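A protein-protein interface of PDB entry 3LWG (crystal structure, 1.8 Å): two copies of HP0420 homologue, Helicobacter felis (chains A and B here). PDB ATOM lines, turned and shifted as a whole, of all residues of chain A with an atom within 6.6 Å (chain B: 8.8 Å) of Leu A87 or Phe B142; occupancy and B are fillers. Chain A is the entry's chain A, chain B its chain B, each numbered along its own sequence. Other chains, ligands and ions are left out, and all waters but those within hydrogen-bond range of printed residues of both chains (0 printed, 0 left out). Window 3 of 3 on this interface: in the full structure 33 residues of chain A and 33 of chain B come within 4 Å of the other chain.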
ATOM      1  N   ASN A  85       5.740 -17.301  31.038  1.00  0.00           N
ATOM      2  CA  ASN A  85       5.712 -16.218  30.070  1.00  0.00           C
ATOM      3  C   ASN A  85       4.286 -16.002  29.577  1.00  0.00           C
ATOM      4  O   ASN A  85       3.616 -16.954  29.112  1.00  0.00           O
ATOM      5  CB  ASN A  85       6.653 -16.507  28.899  1.00  0.00           C
ATOM      6  CG  ASN A  85       8.097 -16.664  29.343  1.00  0.00           C
ATOM      7  OD1 ASN A  85       8.551 -16.006  30.261  1.00  0.00           O
ATOM      8  ND2 ASN A  85       8.820 -17.537  28.680  1.00  0.00           N
ATOM      9  N   LEU A  86       3.813 -14.743  29.678  1.00  0.00           N
ATOM     10  CA  LEU A  86       2.518 -14.403  29.125  1.00  0.00           C
ATOM     11  C   LEU A  86       2.845 -13.835  27.757  1.00  0.00           C
ATOM     12  O   LEU A  86       3.444 -12.773  27.659  1.00  0.00           O
ATOM     13  CB  LEU A  86       1.824 -13.362  30.010  1.00  0.00           C
ATOM     14  CG  LEU A  86       1.672 -13.805  31.481  1.00  0.00           C
ATOM     15  CD1 LEU A  86       0.915 -12.787  32.374  1.00  0.00           C
ATOM     16  CD2 LEU A  86       0.996 -15.155  31.526  1.00  0.00           C
ATOM     17  N   LEU A  87       2.495 -14.552  26.703  1.00  0.00           N
ATOM     18  CA  LEU A  87       3.049 -14.253  25.372  1.00  0.00           C
ATOM     19  C   LEU A  87       2.233 -13.253  24.572  1.00  0.00           C
ATOM     20  O   LEU A  87       2.759 -12.649  23.642  1.00  0.00           O
ATOM     21  CB  LEU A  87       3.218 -15.557  24.545  1.00  0.00           C
ATOM     22  CG  LEU A  87       4.137 -16.560  25.245  1.00  0.00           C
ATOM     23  CD1 LEU A  87       4.194 -17.887  24.489  1.00  0.00           C
ATOM     24  CD2 LEU A  87       5.537 -15.952  25.357  1.00  0.00           C
ATOM     25  N   ALA A  88       0.966 -13.079  24.943  1.00  0.00           N
ATOM     26  CA  ALA A  88       0.110 -12.046  24.357  1.00  0.00           C
ATOM     27  C   ALA A  88      -0.961 -11.673  25.387  1.00  0.00           C
ATOM     28  O   ALA A  88      -1.305 -12.504  26.231  1.00  0.00           O
ATOM     29  CB  ALA A  88      -0.535 -12.600  23.117  1.00  0.00           C
ATOM     30  N   PRO A  89      -1.505 -10.446  25.301  1.00  0.00           N
ATOM     31  CA  PRO A  89      -2.692 -10.083  26.090  1.00  0.00           C
ATOM     32  C   PRO A  89      -3.821 -11.024  25.737  1.00  0.00           C
ATOM     33  O   PRO A  89      -4.037 -11.320  24.570  1.00  0.00           O
ATOM     34  CB  PRO A  89      -3.087  -8.689  25.556  1.00  0.00           C
ATOM     35  CG  PRO A  89      -2.008  -8.237  24.667  1.00  0.00           C
ATOM     36  CD  PRO A  89      -1.068  -9.367  24.392  1.00  0.00           C
ATOM     37  N   GLY A 116      -0.691 -22.561  26.794  1.00  0.00           N
ATOM     38  CA  GLY A 116      -2.016 -22.046  26.484  1.00  0.00           C
ATOM     39  C   GLY A 116      -2.091 -21.530  25.062  1.00  0.00           C
ATOM     40  O   GLY A 116      -1.204 -20.835  24.596  1.00  0.00           O
ATOM     41  N   LYS A 122       0.205 -20.065  20.322  1.00  0.00           N
ATOM     42  CA  LYS A 122       0.638 -20.114  21.718  1.00  0.00           C
ATOM     43  C   LYS A 122       0.560 -18.705  22.302  1.00  0.00           C
ATOM     44  O   LYS A 122       1.175 -17.785  21.774  1.00  0.00           O
ATOM     45  CB  LYS A 122       2.064 -20.694  21.854  1.00  0.00           C
ATOM     46  CG  LYS A 122       2.445 -21.141  23.280  1.00  0.00           C
ATOM     47  CD  LYS A 122       3.952 -21.528  23.411  1.00  0.00           C
ATOM     48  CE  LYS A 122       4.241 -22.841  22.703  1.00  0.00           C
ATOM     49  NZ  LYS A 122       5.684 -23.302  22.808  1.00  0.00           N
ATOM     50  N   VAL A 123      -0.234 -18.534  23.370  1.00  0.00           N
ATOM     51  CA  VAL A 123      -0.288 -17.294  24.078  1.00  0.00           C
ATOM     52  C   VAL A 123       0.224 -17.348  25.526  1.00  0.00           C
ATOM     53  O   VAL A 123       0.263 -16.318  26.195  1.00  0.00           O
ATOM     54  CB  VAL A 123      -1.723 -16.714  24.100  1.00  0.00           C
ATOM     55  CG1 VAL A 123      -2.216 -16.371  22.663  1.00  0.00           C
ATOM     56  CG2 VAL A 123      -2.689 -17.640  24.864  1.00  0.00           C
ATOM     57  N   PHE A 124       0.621 -18.524  25.984  1.00  0.00           N
ATOM     58  CA  PHE A 124       1.013 -18.715  27.375  1.00  0.00           C
ATOM     59  C   PHE A 124       1.969 -19.903  27.391  1.00  0.00           C
ATOM     60  O   PHE A 124       1.691 -20.912  26.744  1.00  0.00           O
ATOM     61  CB  PHE A 124      -0.220 -19.034  28.237  1.00  0.00           C
ATOM     62  CG  PHE A 124       0.131 -19.384  29.674  1.00  0.00           C
ATOM     63  CD1 PHE A 124       0.117 -18.419  30.639  1.00  0.00           C
ATOM     64  CD2 PHE A 124       0.505 -20.690  30.029  1.00  0.00           C
ATOM     65  CE1 PHE A 124       0.470 -18.716  31.941  1.00  0.00           C
ATOM     66  CE2 PHE A 124       0.868 -21.004  31.358  1.00  0.00           C
ATOM     67  CZ  PHE A 124       0.871 -20.016  32.307  1.00  0.00           C
ATOM     68  N   GLU A 125       3.043 -19.813  28.155  1.00  0.00           N
ATOM     69  CA  GLU A 125       3.866 -21.006  28.478  1.00  0.00           C
ATOM     70  C   GLU A 125       4.419 -20.898  29.907  1.00  0.00           C
ATOM     71  O   GLU A 125       4.808 -19.830  30.366  1.00  0.00           O
ATOM     72  CB  GLU A 125       4.977 -21.197  27.420  1.00  0.00           C
ATOM     73  CG  GLU A 125       5.816 -19.956  27.276  1.00  0.00           C
ATOM     74  CD  GLU A 125       6.989 -20.096  26.336  1.00  0.00           C
ATOM     75  OE1 GLU A 125       6.981 -21.081  25.573  1.00  0.00           O
ATOM     76  OE2 GLU A 125       7.898 -19.239  26.385  1.00  0.00           O
ATOM     77  N   ASN B  76      -0.571   1.898  30.131  1.00  0.00           N
ATOM     78  CA  ASN B  76      -0.284   0.993  29.034  1.00  0.00           C
ATOM     79  C   ASN B  76       0.747  -0.073  29.373  1.00  0.00           C
ATOM     80  O   ASN B  76       1.525  -0.497  28.512  1.00  0.00           O
ATOM     81  CB  ASN B  76       0.199   1.788  27.818  1.00  0.00           C
ATOM     82  CG  ASN B  76      -0.838   2.727  27.286  1.00  0.00           C
ATOM     83  OD1 ASN B  76      -1.964   2.803  27.764  1.00  0.00           O
ATOM     84  ND2 ASN B  76      -0.459   3.450  26.257  1.00  0.00           N
ATOM     85  N   LEU B  78       1.718  -4.012  30.927  1.00  0.00           N
ATOM     86  CA  LEU B  78       1.205  -5.299  31.384  1.00  0.00           C
ATOM     87  C   LEU B  78       2.290  -6.247  31.800  1.00  0.00           C
ATOM     88  O   LEU B  78       3.472  -6.103  31.451  1.00  0.00           O
ATOM     89  CB  LEU B  78       0.249  -5.978  30.387  1.00  0.00           C
ATOM     90  CG  LEU B  78       0.771  -5.993  28.959  1.00  0.00           C
ATOM     91  CD1 LEU B  78       1.986  -6.803  28.928  1.00  0.00           C
ATOM     92  CD2 LEU B  78      -0.265  -6.521  27.968  1.00  0.00           C
ATOM     93  N   ILE B  79       1.866  -7.232  32.565  1.00  0.00           N
ATOM     94  CA  ILE B  79       2.801  -8.225  33.027  1.00  0.00           C
ATOM     95  C   ILE B  79       3.185  -9.117  31.864  1.00  0.00           C
ATOM     96  O   ILE B  79       2.290  -9.675  31.200  1.00  0.00           O
ATOM     97  CB  ILE B  79       2.188  -9.167  34.103  1.00  0.00           C
ATOM     98  CG1 ILE B  79       1.681  -8.368  35.329  1.00  0.00           C
ATOM     99  CG2 ILE B  79       3.244 -10.159  34.482  1.00  0.00           C
ATOM    100  CD1 ILE B  79       2.748  -7.911  36.209  1.00  0.00           C
ATOM    101  N   SER B  80       4.482  -9.303  31.645  1.00  0.00           N
ATOM    102  CA  SER B  80       4.913 -10.161  30.554  1.00  0.00           C
ATOM    103  C   SER B  80       5.482 -11.512  31.000  1.00  0.00           C
ATOM    104  O   SER B  80       5.457 -12.466  30.239  1.00  0.00           O
ATOM    105  CB  SER B  80       5.925  -9.455  29.655  1.00  0.00           C
ATOM    106  OG  SER B  80       7.065  -9.062  30.420  1.00  0.00           O
ATOM    107  N   SER B  81       6.019 -11.591  32.212  1.00  0.00           N
ATOM    108  CA  SER B  81       6.710 -12.808  32.645  1.00  0.00           C
ATOM    109  C   SER B  81       6.792 -12.810  34.148  1.00  0.00           C
ATOM    110  O   SER B  81       6.750 -11.743  34.735  1.00  0.00           O
ATOM    111  CB  SER B  81       8.156 -12.799  32.098  1.00  0.00           C
ATOM    112  OG  SER B  81       8.727 -14.074  32.352  1.00  0.00           O
ATOM    113  N   LEU B 131       6.026  -4.848  30.756  1.00  0.00           N
ATOM    114  CA  LEU B 131       6.343  -4.117  29.544  1.00  0.00           C
ATOM    115  C   LEU B 131       5.379  -2.955  29.405  1.00  0.00           C
ATOM    116  O   LEU B 131       4.228  -3.058  29.803  1.00  0.00           O
ATOM    117  CB  LEU B 131       6.195  -5.050  28.343  1.00  0.00           C
ATOM    118  CG  LEU B 131       7.187  -6.204  28.314  1.00  0.00           C
ATOM    119  CD1 LEU B 131       6.831  -7.149  27.142  1.00  0.00           C
ATOM    120  CD2 LEU B 131       8.615  -5.710  28.202  1.00  0.00           C
ATOM    121  N   VAL B 132       5.861  -1.852  28.816  1.00  0.00           N
ATOM    122  CA  VAL B 132       5.044  -0.663  28.575  1.00  0.00           C
ATOM    123  C   VAL B 132       4.933  -0.440  27.073  1.00  0.00           C
ATOM    124  O   VAL B 132       5.957  -0.448  26.366  1.00  0.00           O
ATOM    125  CB  VAL B 132       5.708   0.564  29.162  1.00  0.00           C
ATOM    126  CG1 VAL B 132       4.821   1.817  28.945  1.00  0.00           C
ATOM    127  CG2 VAL B 132       5.982   0.339  30.655  1.00  0.00           C
ATOM    128  N   PHE B 133       3.697  -0.290  26.594  1.00  0.00           N
ATOM    129  CA  PHE B 133       3.418  -0.153  25.154  1.00  0.00           C
ATOM    130  C   PHE B 133       2.914   1.216  24.735  1.00  0.00           C
ATOM    131  O   PHE B 133       2.382   1.967  25.530  1.00  0.00           O
ATOM    132  CB  PHE B 133       2.388  -1.192  24.731  1.00  0.00           C
ATOM    133  CG  PHE B 133       2.882  -2.581  24.893  1.00  0.00           C
ATOM    134  CD1 PHE B 133       2.624  -3.293  26.058  1.00  0.00           C
ATOM    135  CD2 PHE B 133       3.647  -3.163  23.913  1.00  0.00           C
ATOM    136  CE1 PHE B 133       3.094  -4.577  26.198  1.00  0.00           C
ATOM    137  CE2 PHE B 133       4.116  -4.455  24.068  1.00  0.00           C
ATOM    138  CZ  PHE B 133       3.837  -5.151  25.208  1.00  0.00           C
ATOM    139  N   LYS B 135       0.662   1.677  22.033  1.00  0.00           N
ATOM    140  CA  LYS B 135      -0.703   1.646  21.472  1.00  0.00           C
ATOM    141  C   LYS B 135      -1.660   0.852  22.345  1.00  0.00           C
ATOM    142  O   LYS B 135      -1.242  -0.101  23.028  1.00  0.00           O
ATOM    143  CB  LYS B 135      -0.719   1.024  20.075  1.00  0.00           C
ATOM    144  CG  LYS B 135       0.219   1.677  19.075  1.00  0.00           C
ATOM    145  CD  LYS B 135       0.344   0.791  17.870  1.00  0.00           C
ATOM    146  CE  LYS B 135       1.661   1.006  17.135  1.00  0.00           C
ATOM    147  NZ  LYS B 135       1.695   0.190  15.878  1.00  0.00           N
ATOM    148  N   PRO B 137      -5.905  -0.611  21.754  1.00  0.00           N
ATOM    149  CA  PRO B 137      -5.801  -1.740  22.697  1.00  0.00           C
ATOM    150  C   PRO B 137      -4.477  -2.520  22.548  1.00  0.00           C
ATOM    151  O   PRO B 137      -3.796  -2.433  21.524  1.00  0.00           O
ATOM    152  CB  PRO B 137      -6.999  -2.625  22.317  1.00  0.00           C
ATOM    153  CG  PRO B 137      -7.383  -2.179  20.923  1.00  0.00           C
ATOM    154  CD  PRO B 137      -7.066  -0.733  20.858  1.00  0.00           C
ATOM    155  N   PHE B 138      -4.123  -3.274  23.577  1.00  0.00           N
ATOM    156  CA  PHE B 138      -2.824  -3.931  23.623  1.00  0.00           C
ATOM    157  C   PHE B 138      -2.543  -4.798  22.442  1.00  0.00           C
ATOM    158  O   PHE B 138      -1.398  -4.936  22.046  1.00  0.00           O
ATOM    159  CB  PHE B 138      -2.704  -4.773  24.898  1.00  0.00           C
ATOM    160  CG  PHE B 138      -2.440  -3.954  26.119  1.00  0.00           C
ATOM    161  CD1 PHE B 138      -1.264  -3.227  26.237  1.00  0.00           C
ATOM    162  CD2 PHE B 138      -3.352  -3.927  27.175  1.00  0.00           C
ATOM    163  CE1 PHE B 138      -1.008  -2.466  27.401  1.00  0.00           C
ATOM    164  CE2 PHE B 138      -3.104  -3.183  28.328  1.00  0.00           C
ATOM    165  CZ  PHE B 138      -1.922  -2.457  28.441  1.00  0.00           C
ATOM    166  N   LYS B 139      -3.585  -5.427  21.903  1.00  0.00           N
ATOM    167  CA  LYS B 139      -3.362  -6.379  20.838  1.00  0.00           C
ATOM    168  C   LYS B 139      -2.695  -5.714  19.613  1.00  0.00           C
ATOM    169  O   LYS B 139      -2.036  -6.412  18.846  1.00  0.00           O
ATOM    170  CB  LYS B 139      -4.667  -7.097  20.451  1.00  0.00           C
ATOM    171  CG  LYS B 139      -5.692  -6.171  19.826  1.00  0.00           C
ATOM    172  CD  LYS B 139      -6.960  -6.902  19.423  1.00  0.00           C
ATOM    173  CE  LYS B 139      -8.105  -5.887  19.277  1.00  0.00           C
ATOM    174  NZ  LYS B 139      -9.206  -6.356  18.357  1.00  0.00           N
ATOM    175  N   PHE B 140      -2.828  -4.389  19.458  1.00  0.00           N
ATOM    176  CA  PHE B 140      -2.237  -3.685  18.295  1.00  0.00           C
ATOM    177  C   PHE B 140      -0.704  -3.729  18.290  1.00  0.00           C
ATOM    178  O   PHE B 140      -0.050  -3.471  17.272  1.00  0.00           O
ATOM    179  CB  PHE B 140      -2.672  -2.226  18.253  1.00  0.00           C
ATOM    180  CG  PHE B 140      -4.110  -2.039  17.825  1.00  0.00           C
ATOM    181  CD1 PHE B 140      -4.767  -0.811  18.010  1.00  0.00           C
ATOM    182  CD2 PHE B 140      -4.807  -3.108  17.257  1.00  0.00           C
ATOM    183  CE1 PHE B 140      -6.120  -0.653  17.602  1.00  0.00           C
ATOM    184  CE2 PHE B 140      -6.149  -2.966  16.878  1.00  0.00           C
ATOM    185  CZ  PHE B 140      -6.798  -1.732  17.045  1.00  0.00           C
ATOM    186  N   ASN B 141      -0.144  -4.054  19.450  1.00  0.00           N
ATOM    187  CA  ASN B 141       1.295  -4.083  19.623  1.00  0.00           C
ATOM    188  C   ASN B 141       1.892  -5.431  19.267  1.00  0.00           C
ATOM    189  O   ASN B 141       3.110  -5.601  19.317  1.00  0.00           O
ATOM    190  CB  ASN B 141       1.615  -3.779  21.078  1.00  0.00           C
ATOM    191  CG  ASN B 141       1.068  -2.456  21.522  1.00  0.00           C
ATOM    192  OD1 ASN B 141       0.065  -2.387  22.252  1.00  0.00           O
ATOM    193  ND2 ASN B 141       1.717  -1.385  21.100  1.00  0.00           N
ATOM    194  N   PHE B 142       1.042  -6.401  18.934  1.00  0.00           N
ATOM    195  CA  PHE B 142       1.514  -7.756  18.647  1.00  0.00           C
ATOM    196  C   PHE B 142       1.067  -8.155  17.247  1.00  0.00           C
ATOM    197  O   PHE B 142       0.308  -7.402  16.621  1.00  0.00           O
ATOM    198  CB  PHE B 142       0.970  -8.776  19.656  1.00  0.00           C
ATOM    199  CG  PHE B 142       1.341  -8.484  21.088  1.00  0.00           C
ATOM    200  CD1 PHE B 142       0.761  -7.402  21.770  1.00  0.00           C
ATOM    201  CD2 PHE B 142       2.266  -9.287  21.760  1.00  0.00           C
ATOM    202  CE1 PHE B 142       1.117  -7.122  23.087  1.00  0.00           C
ATOM    203  CE2 PHE B 142       2.598  -9.041  23.079  1.00  0.00           C
ATOM    204  CZ  PHE B 142       2.050  -7.964  23.743  1.00  0.00           C
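Among the printed residues, pairs that only touch across the chains: Asn A85 with Ser B80, Leu A86 with Ile B79, Leu A87 with Phe B142, Pro A89 with Phe B138 and Pro A89 with Phe B142.
Leu A87 touches just one residue of chain B: Phe B142 (3.7 Å). Phe B142 touches just these residues of chain A: Leu A87 and Pro A89. No residue of chain B comes within 4 Å of Ala A88. Printed residues of chain A within 4 Å of Ser B80: Asn A85 and Leu A86. Of the printed residues of chain B, Leu A86 touches Ile B79 and Ser B80. Of the printed residues of chain A, Ile B79 touches Leu A86 (3.6 Å). Of the printed residues of chain B, Pro A89 touches Phe B138 (3.5 Å) and Phe B142 (3.4 Å).
The backbone NH of Asn A85 sits at hydrogen-bond distance from the backbone carbonyl oxygen of Glu A125 (2.8 Å). N of Leu A87 is in hydrogen-bond range of O of Val A123 (2.9 Å). The backbone carbonyl oxygen (O) of Phe B138 lies close to the side-chain amide oxygen (OD1) of Asn B141, at 2.9 Å.
Of the 10 printed residues of chain A, 4 touch a printed residue of chain B. Hydrophobic or aromatic side chains of chain B that line the printed part of chain A: Phe B138 and Phe B142. Among the printed residues, 7 pairs touch across the chains. Among the printed residues, no Asp or Glu carboxylate lies within 4 Å of a Lys or Arg side-chain nitrogen of the other chain.
No position is printed for both chains. Of the 7 pairs that touch across the chains among the printed residues, none has its exchanged pair printed and touching as well.
OG of Ser B81 lies within hydrogen-bond range of OD1 of Asn A85 (2.9 Å). N of Leu A86 is in hydrogen-bond range of O of Ser B80 (2.9 Å).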
